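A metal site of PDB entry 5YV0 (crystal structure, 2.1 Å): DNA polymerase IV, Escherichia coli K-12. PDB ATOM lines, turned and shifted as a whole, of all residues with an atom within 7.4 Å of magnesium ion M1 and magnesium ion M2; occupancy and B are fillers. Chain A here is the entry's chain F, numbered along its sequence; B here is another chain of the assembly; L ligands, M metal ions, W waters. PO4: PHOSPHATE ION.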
ATOM      1  N   HIS A   7       2.997  12.858  24.867  1.00  0.00           N
ATOM      2  CA  HIS A   7       2.077  12.291  23.886  1.00  0.00           C
ATOM      3  C   HIS A   7       0.673  12.328  24.467  1.00  0.00           C
ATOM      4  O   HIS A   7       0.427  11.716  25.516  1.00  0.00           O
ATOM      5  CB  HIS A   7       2.481  10.865  23.515  1.00  0.00           C
ATOM      6  CG  HIS A   7       1.584  10.255  22.491  1.00  0.00           C
ATOM      7  ND1 HIS A   7       0.592   9.355  22.810  1.00  0.00           N
ATOM      8  CD2 HIS A   7       1.527  10.438  21.150  1.00  0.00           C
ATOM      9  CE1 HIS A   7      -0.037   8.996  21.703  1.00  0.00           C
ATOM     10  NE2 HIS A   7       0.515   9.633  20.673  1.00  0.00           N
ATOM     11  N   VAL A   8      -0.235  13.048  23.799  1.00  0.00           N
ATOM     12  CA  VAL A   8      -1.638  13.164  24.214  1.00  0.00           C
ATOM     13  C   VAL A   8      -2.474  12.307  23.278  1.00  0.00           C
ATOM     14  O   VAL A   8      -2.272  12.335  22.064  1.00  0.00           O
ATOM     15  CB  VAL A   8      -2.114  14.623  24.191  1.00  0.00           C
ATOM     16  CG1 VAL A   8      -3.571  14.716  24.651  1.00  0.00           C
ATOM     17  CG2 VAL A   8      -1.191  15.522  25.048  1.00  0.00           C
ATOM     18  N   ASP A   9      -3.430  11.566  23.851  1.00  0.00           N
ATOM     19  CA  ASP A   9      -4.199  10.569  23.093  1.00  0.00           C
ATOM     20  C   ASP A   9      -5.630  10.507  23.604  1.00  0.00           C
ATOM     21  O   ASP A   9      -5.847  10.179  24.765  1.00  0.00           O
ATOM     22  CB  ASP A   9      -3.547   9.189  23.214  1.00  0.00           C
ATOM     23  CG  ASP A   9      -4.044   8.226  22.143  1.00  0.00           C
ATOM     24  OD1 ASP A   9      -4.664   8.676  21.163  1.00  0.00           O
ATOM     25  OD2 ASP A   9      -3.771   7.007  22.273  1.00  0.00           O
ATOM     26  N   MET A  10      -6.602  10.777  22.724  1.00  0.00           N
ATOM     27  CA  MET A  10      -8.014  10.739  23.126  1.00  0.00           C
ATOM     28  C   MET A  10      -8.443   9.310  23.416  1.00  0.00           C
ATOM     29  O   MET A  10      -7.978   8.368  22.773  1.00  0.00           O
ATOM     30  CB  MET A  10      -8.910  11.341  22.053  1.00  0.00           C
ATOM     31  CG  MET A  10      -8.592  12.774  21.687  1.00  0.00           C
ATOM     32  SD  MET A  10      -8.696  13.950  23.028  1.00  0.00           S
ATOM     33  CE  MET A  10     -10.458  14.003  23.311  1.00  0.00           C
ATOM     34  N   ASP A  11      -9.305   9.147  24.432  1.00  0.00           N
ATOM     35  CA  ASP A  11      -9.822   7.833  24.806  1.00  0.00           C
ATOM     36  C   ASP A  11     -11.007   7.441  23.914  1.00  0.00           C
ATOM     37  O   ASP A  11     -11.958   8.216  23.779  1.00  0.00           O
ATOM     38  CB  ASP A  11     -10.289   7.823  26.266  1.00  0.00           C
ATOM     39  CG  ASP A  11      -9.191   8.213  27.246  1.00  0.00           C
ATOM     40  OD1 ASP A  11      -8.064   7.674  27.161  1.00  0.00           O
ATOM     41  OD2 ASP A  11      -9.480   9.051  28.130  1.00  0.00           O
ATOM     42  N   CYS A  12     -10.960   6.236  23.349  1.00  0.00           N
ATOM     43  CA  CYS A  12     -12.031   5.658  22.523  1.00  0.00           C
ATOM     44  C   CYS A  12     -12.636   6.715  21.598  1.00  0.00           C
ATOM     45  O   CYS A  12     -13.859   6.903  21.546  1.00  0.00           O
ATOM     46  CB  CYS A  12     -13.099   4.996  23.388  1.00  0.00           C
ATOM     47  SG  CYS A  12     -12.399   3.659  24.384  1.00  0.00           S
ATOM     48  N   PHE A  13     -11.743   7.412  20.873  1.00  0.00           N
ATOM     49  CA  PHE A  13     -12.059   8.707  20.298  1.00  0.00           C
ATOM     50  C   PHE A  13     -13.414   8.750  19.583  1.00  0.00           C
ATOM     51  O   PHE A  13     -14.303   9.528  19.972  1.00  0.00           O
ATOM     52  CB  PHE A  13     -10.934   9.133  19.346  1.00  0.00           C
ATOM     53  CG  PHE A  13     -11.138  10.499  18.776  1.00  0.00           C
ATOM     54  CD1 PHE A  13     -11.539  11.534  19.612  1.00  0.00           C
ATOM     55  CD2 PHE A  13     -10.974  10.742  17.427  1.00  0.00           C
ATOM     56  CE1 PHE A  13     -11.756  12.791  19.096  1.00  0.00           C
ATOM     57  CE2 PHE A  13     -11.193  11.999  16.889  1.00  0.00           C
ATOM     58  CZ  PHE A  13     -11.575  13.038  17.713  1.00  0.00           C
ATOM     59  N   PHE A  14     -13.582   7.982  18.499  1.00  0.00           N
ATOM     60  CA  PHE A  14     -14.836   8.089  17.749  1.00  0.00           C
ATOM     61  C   PHE A  14     -16.028   7.755  18.643  1.00  0.00           C
ATOM     62  O   PHE A  14     -17.068   8.434  18.583  1.00  0.00           O
ATOM     63  CB  PHE A  14     -14.879   7.160  16.533  1.00  0.00           C
ATOM     64  CG  PHE A  14     -13.930   7.499  15.416  1.00  0.00           C
ATOM     65  CD1 PHE A  14     -13.008   8.530  15.524  1.00  0.00           C
ATOM     66  CD2 PHE A  14     -13.958   6.766  14.231  1.00  0.00           C
ATOM     67  CE1 PHE A  14     -12.114   8.803  14.479  1.00  0.00           C
ATOM     68  CE2 PHE A  14     -13.093   7.025  13.192  1.00  0.00           C
ATOM     69  CZ  PHE A  14     -12.162   8.066  13.304  1.00  0.00           C
ATOM     70  N   THR A  44     -13.589   1.489  16.141  1.00  0.00           N
ATOM     71  CA  THR A  44     -13.302   1.499  17.562  1.00  0.00           C
ATOM     72  C   THR A  44     -14.612   1.209  18.278  1.00  0.00           C
ATOM     73  O   THR A  44     -15.688   1.181  17.674  1.00  0.00           O
ATOM     74  CB  THR A  44     -12.701   2.824  18.012  1.00  0.00           C
ATOM     75  OG1 THR A  44     -12.197   2.700  19.330  1.00  0.00           O
ATOM     76  CG2 THR A  44     -13.762   3.910  17.963  1.00  0.00           C
ATOM     77  N   ARG A  50     -15.830  -3.280  24.556  1.00  0.00           N
ATOM     78  CA  ARG A  50     -14.513  -3.913  24.724  1.00  0.00           C
ATOM     79  C   ARG A  50     -14.512  -4.988  25.801  1.00  0.00           C
ATOM     80  O   ARG A  50     -13.748  -5.950  25.717  1.00  0.00           O
ATOM     81  CB  ARG A  50     -13.456  -2.863  25.109  1.00  0.00           C
ATOM     82  CG  ARG A  50     -13.178  -1.863  24.018  1.00  0.00           C
ATOM     83  CD  ARG A  50     -12.236  -0.764  24.533  1.00  0.00           C
ATOM     84  NE  ARG A  50     -12.011   0.240  23.500  1.00  0.00           N
ATOM     85  CZ  ARG A  50     -11.193   0.085  22.473  1.00  0.00           C
ATOM     86  NH1 ARG A  50     -10.498  -1.039  22.349  1.00  0.00           N
ATOM     87  NH2 ARG A  50     -11.075   1.039  21.565  1.00  0.00           N
ATOM     88  N   LEU A 101      -0.236  13.006  14.937  1.00  0.00           N
ATOM     89  CA  LEU A 101      -0.012  11.708  14.308  1.00  0.00           C
ATOM     90  C   LEU A 101      -1.269  11.142  13.658  1.00  0.00           C
ATOM     91  O   LEU A 101      -1.150  10.232  12.833  1.00  0.00           O
ATOM     92  CB  LEU A 101       0.514  10.696  15.324  1.00  0.00           C
ATOM     93  CG  LEU A 101       1.723  11.239  16.085  1.00  0.00           C
ATOM     94  CD1 LEU A 101       2.018  10.407  17.323  1.00  0.00           C
ATOM     95  CD2 LEU A 101       2.924  11.266  15.139  1.00  0.00           C
ATOM     96  N   SER A 102      -2.444  11.632  14.025  1.00  0.00           N
ATOM     97  CA  SER A 102      -3.753  11.207  13.538  1.00  0.00           C
ATOM     98  C   SER A 102      -4.728  12.258  14.061  1.00  0.00           C
ATOM     99  O   SER A 102      -4.306  13.257  14.659  1.00  0.00           O
ATOM    100  CB  SER A 102      -4.094   9.787  13.991  1.00  0.00           C
ATOM    101  OG  SER A 102      -4.151   9.686  15.404  1.00  0.00           O
ATOM    102  N   LEU A 103      -6.026  12.048  13.843  1.00  0.00           N
ATOM    103  CA  LEU A 103      -7.003  13.019  14.348  1.00  0.00           C
ATOM    104  C   LEU A 103      -6.831  13.269  15.847  1.00  0.00           C
ATOM    105  O   LEU A 103      -6.877  14.416  16.304  1.00  0.00           O
ATOM    106  CB  LEU A 103      -8.423  12.535  14.072  1.00  0.00           C
ATOM    107  CG  LEU A 103      -8.848  12.578  12.617  1.00  0.00           C
ATOM    108  CD1 LEU A 103     -10.298  12.173  12.536  1.00  0.00           C
ATOM    109  CD2 LEU A 103      -8.626  13.968  12.057  1.00  0.00           C
ATOM    110  N   ASP A 104      -6.617  12.202  16.624  1.00  0.00           N
ATOM    111  CA  ASP A 104      -6.881  12.224  18.059  1.00  0.00           C
ATOM    112  C   ASP A 104      -5.626  12.215  18.926  1.00  0.00           C
ATOM    113  O   ASP A 104      -5.740  12.011  20.146  1.00  0.00           O
ATOM    114  CB  ASP A 104      -7.804  11.047  18.440  1.00  0.00           C
ATOM    115  CG  ASP A 104      -7.041   9.796  18.835  1.00  0.00           C
ATOM    116  OD1 ASP A 104      -6.017   9.474  18.194  1.00  0.00           O
ATOM    117  OD2 ASP A 104      -7.447   9.144  19.812  1.00  0.00           O
ATOM    118  N   GLU A 105      -4.443  12.437  18.351  1.00  0.00           N
ATOM    119  CA  GLU A 105      -3.232  12.342  19.140  1.00  0.00           C
ATOM    120  C   GLU A 105      -2.131  13.200  18.529  1.00  0.00           C
ATOM    121  O   GLU A 105      -2.165  13.512  17.330  1.00  0.00           O
ATOM    122  CB  GLU A 105      -2.786  10.874  19.295  1.00  0.00           C
ATOM    123  CG  GLU A 105      -2.104  10.241  18.111  1.00  0.00           C
ATOM    124  CD  GLU A 105      -1.774   8.771  18.357  1.00  0.00           C
ATOM    125  OE1 GLU A 105      -2.709   7.968  18.582  1.00  0.00           O
ATOM    126  OE2 GLU A 105      -0.585   8.388  18.317  1.00  0.00           O
ATOM    127  N   ALA A 106      -1.198  13.617  19.370  1.00  0.00           N
ATOM    128  CA  ALA A 106      -0.058  14.427  18.953  1.00  0.00           C
ATOM    129  C   ALA A 106       1.094  14.216  19.912  1.00  0.00           C
ATOM    130  O   ALA A 106       0.892  13.899  21.085  1.00  0.00           O
ATOM    131  CB  ALA A 106      -0.388  15.922  18.918  1.00  0.00           C
ATOM    132  N   LYS A 151       4.818   7.763  23.846  1.00  0.00           N
ATOM    133  CA  LYS A 151       3.649   7.178  23.208  1.00  0.00           C
ATOM    134  C   LYS A 151       3.264   5.863  23.889  1.00  0.00           C
ATOM    135  O   LYS A 151       2.084   5.591  24.110  1.00  0.00           O
ATOM    136  CB  LYS A 151       3.898   6.990  21.697  1.00  0.00           C
ATOM    137  CG  LYS A 151       2.730   6.267  20.977  1.00  0.00           C
ATOM    138  CD  LYS A 151       2.787   6.577  19.448  1.00  0.00           C
ATOM    139  CE  LYS A 151       1.796   5.694  18.664  1.00  0.00           C
ATOM    140  NZ  LYS A 151       0.356   5.888  19.024  1.00  0.00           N
ATOM    141  N   ASP A 155      -0.527   4.977  26.797  1.00  0.00           N
ATOM    142  CA  ASP A 155      -1.401   3.816  26.837  1.00  0.00           C
ATOM    143  C   ASP A 155      -1.543   3.204  28.219  1.00  0.00           C
ATOM    144  O   ASP A 155      -2.531   2.498  28.471  1.00  0.00           O
ATOM    145  CB  ASP A 155      -0.889   2.739  25.893  1.00  0.00           C
ATOM    146  CG  ASP A 155      -1.652   2.688  24.618  1.00  0.00           C
ATOM    147  OD1 ASP A 155      -2.373   3.676  24.326  1.00  0.00           O
ATOM    148  OD2 ASP A 155      -1.545   1.666  23.905  1.00  0.00           O
ATOM    149  N   LYS A 158      -4.564   4.628  30.669  1.00  0.00           N
ATOM    150  CA  LYS A 158      -5.807   5.091  30.072  1.00  0.00           C
ATOM    151  C   LYS A 158      -6.976   4.187  30.523  1.00  0.00           C
ATOM    152  O   LYS A 158      -6.753   3.050  30.926  1.00  0.00           O
ATOM    153  CB  LYS A 158      -5.677   5.226  28.532  1.00  0.00           C
ATOM    154  CG  LYS A 158      -5.669   3.997  27.670  1.00  0.00           C
ATOM    155  CD  LYS A 158      -5.892   4.419  26.177  1.00  0.00           C
ATOM    156  CE  LYS A 158      -5.207   5.773  25.804  1.00  0.00           C
ATOM    157  NZ  LYS A 158      -6.137   6.852  25.233  1.00  0.00           N
ATOM    158  P    DC B  18      -1.058   3.247  16.603  1.00  0.00           P
ATOM    159  OP1  DC B  18      -0.728   3.876  17.889  1.00  0.00           O
ATOM    160  OP2  DC B  18      -1.426   1.814  16.565  1.00  0.00           O
ATOM    161  O5'  DC B  18      -2.259   4.094  15.973  1.00  0.00           O
ATOM    162  C5'  DC B  18      -2.202   5.521  16.010  1.00  0.00           C
ATOM    163  C4'  DC B  18      -3.435   6.103  15.368  1.00  0.00           C
ATOM    164  O4'  DC B  18      -3.444   5.763  13.949  1.00  0.00           O
ATOM    165  C3'  DC B  18      -4.743   5.550  15.894  1.00  0.00           C
ATOM    166  O3'  DC B  18      -5.133   6.210  17.081  1.00  0.00           O
ATOM    167  C2'  DC B  18      -5.694   5.832  14.734  1.00  0.00           C
ATOM    168  C1'  DC B  18      -4.776   5.593  13.514  1.00  0.00           C
ATOM    169  N1   DC B  18      -4.899   4.244  12.904  1.00  0.00           N
ATOM    170  C2   DC B  18      -5.869   4.043  11.950  1.00  0.00           C
ATOM    171  O2   DC B  18      -6.625   4.985  11.679  1.00  0.00           O
ATOM    172  N3   DC B  18      -5.973   2.816  11.348  1.00  0.00           N
ATOM    173  C4   DC B  18      -5.123   1.843  11.701  1.00  0.00           C
ATOM    174  N4   DC B  18      -5.254   0.660  11.097  1.00  0.00           N
ATOM    175  C5   DC B  18      -4.132   2.032  12.707  1.00  0.00           C
ATOM    176  C6   DC B  18      -4.036   3.243  13.260  1.00  0.00           C
ATOM    177  P    DT B  19      -6.081   5.464  18.161  1.00  0.00           P
ATOM    178  OP1  DT B  19      -6.085   6.255  19.434  1.00  0.00           O
ATOM    179  OP2  DT B  19      -5.676   4.037  18.171  1.00  0.00           O
ATOM    180  O5'  DT B  19      -7.523   5.535  17.489  1.00  0.00           O
ATOM    181  C5'  DT B  19      -8.174   6.803  17.277  1.00  0.00           C
ATOM    182  C4'  DT B  19      -9.403   6.624  16.381  1.00  0.00           C
ATOM    183  O4'  DT B  19      -8.977   6.177  15.070  1.00  0.00           O
ATOM    184  C3'  DT B  19     -10.378   5.529  16.851  1.00  0.00           C
ATOM    185  O3'  DT B  19     -11.303   6.035  17.776  1.00  0.00           O
ATOM    186  C2'  DT B  19     -11.086   5.169  15.561  1.00  0.00           C
ATOM    187  C1'  DT B  19      -9.941   5.272  14.535  1.00  0.00           C
ATOM    188  N1   DT B  19      -9.299   3.941  14.239  1.00  0.00           N
ATOM    189  C2   DT B  19      -9.722   3.258  13.131  1.00  0.00           C
ATOM    190  O2   DT B  19     -10.560   3.687  12.389  1.00  0.00           O
ATOM    191  N3   DT B  19      -9.114   2.050  12.938  1.00  0.00           N
ATOM    192  C4   DT B  19      -8.143   1.467  13.727  1.00  0.00           C
ATOM    193  O4   DT B  19      -7.655   0.357  13.477  1.00  0.00           O
ATOM    194  C5   DT B  19      -7.767   2.224  14.902  1.00  0.00           C
ATOM    195  C7   DT B  19      -6.722   1.680  15.874  1.00  0.00           C
ATOM    196  C6   DT B  19      -8.363   3.417  15.094  1.00  0.00           C
HETATM  197  P   PO4 L   1      -9.335   4.672  20.379  1.00  0.00           P
HETATM  198  O1  PO4 L   1      -9.032   6.127  20.602  1.00  0.00           O
HETATM  199  O2  PO4 L   1     -10.610   4.550  19.612  1.00  0.00           O
HETATM  200  O3  PO4 L   1      -8.121   3.937  19.833  1.00  0.00           O
HETATM  201  O4  PO4 L   1      -9.869   3.919  21.577  1.00  0.00           O
HETATM  202 MG    MG M   1      -4.739   7.990  18.990  1.00  0.00          MG
HETATM  203 MG    MG M   2      -7.081   7.165  21.067  1.00  0.00          MG
HETATM  204  O   HOH W   1      -2.652   5.805  19.767  1.00  0.00           O
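Of the 21 residues printed, 4 come within 4 Å of magnesium ion M2.
The nearest printed residue that does not touch magnesium ion M2 is Lys 158 (4.3 Å).
OE1 of Glu 105 binds magnesium ion M1 (2.1 Å).
OD1 of Asp 104 is bound to magnesium ion M1 (2.1 Å).
Magnesium ion M1 is bound by OP1 of DT 19 of chain B (2.2 Å).
Magnesium ion M1 is bound by the side-chain carboxylate (OD1) of Asp 9 (2.3 Å).
Magnesium ion M1 has four donor atoms within binding distance.
Slightly farther from magnesium ion M1 lies O3' of DC 18 of chain B (2.6 Å).
NZ of Lys 151 is in salt-bridge range of OE2 of Glu 105, 2.8 Å away.
The side-chain carboxylate of Glu 105 is in hydrogen-bond range of a ring nitrogen (NE2) of His 7 (2.9 Å).
OD1 of Asp 104 lies close to OG of Ser 102, 3.4 Å away.
The backbone NH (N) of Phe 13 is in hydrogen-bond range of O3' of DT 19 of chain B (3.4 Å).
O3' of DT 19 of chain B sits at hydrogen-bond distance from the backbone NH (N) of Phe 14 (3.1 Å).
O of Met 10 lies close to NZ of Lys 158 (3.4 Å).
The side-chain carboxylate (OD2) of Asp 9 lies within salt-bridge range of the side-chain amino group (NZ) of Lys 158 (3.8 Å).
OP1 of DC 18 of chain B lies within salt-bridge range of the side-chain amino group (NZ) of Lys 151 (2.6 Å).
Water W1 lies within hydrogen-bond range of OD2 of Asp 9, NZ of Lys 151 and OP1 of DC 18 of chain B.
Magnesium ion M2 is bound by OP1 of DT 19 of chain B (2.1 Å), O1 of the ligand (2.3 Å), O of Met 10 (2.3 Å) and OD2 of Asp 104 (2.4 Å).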
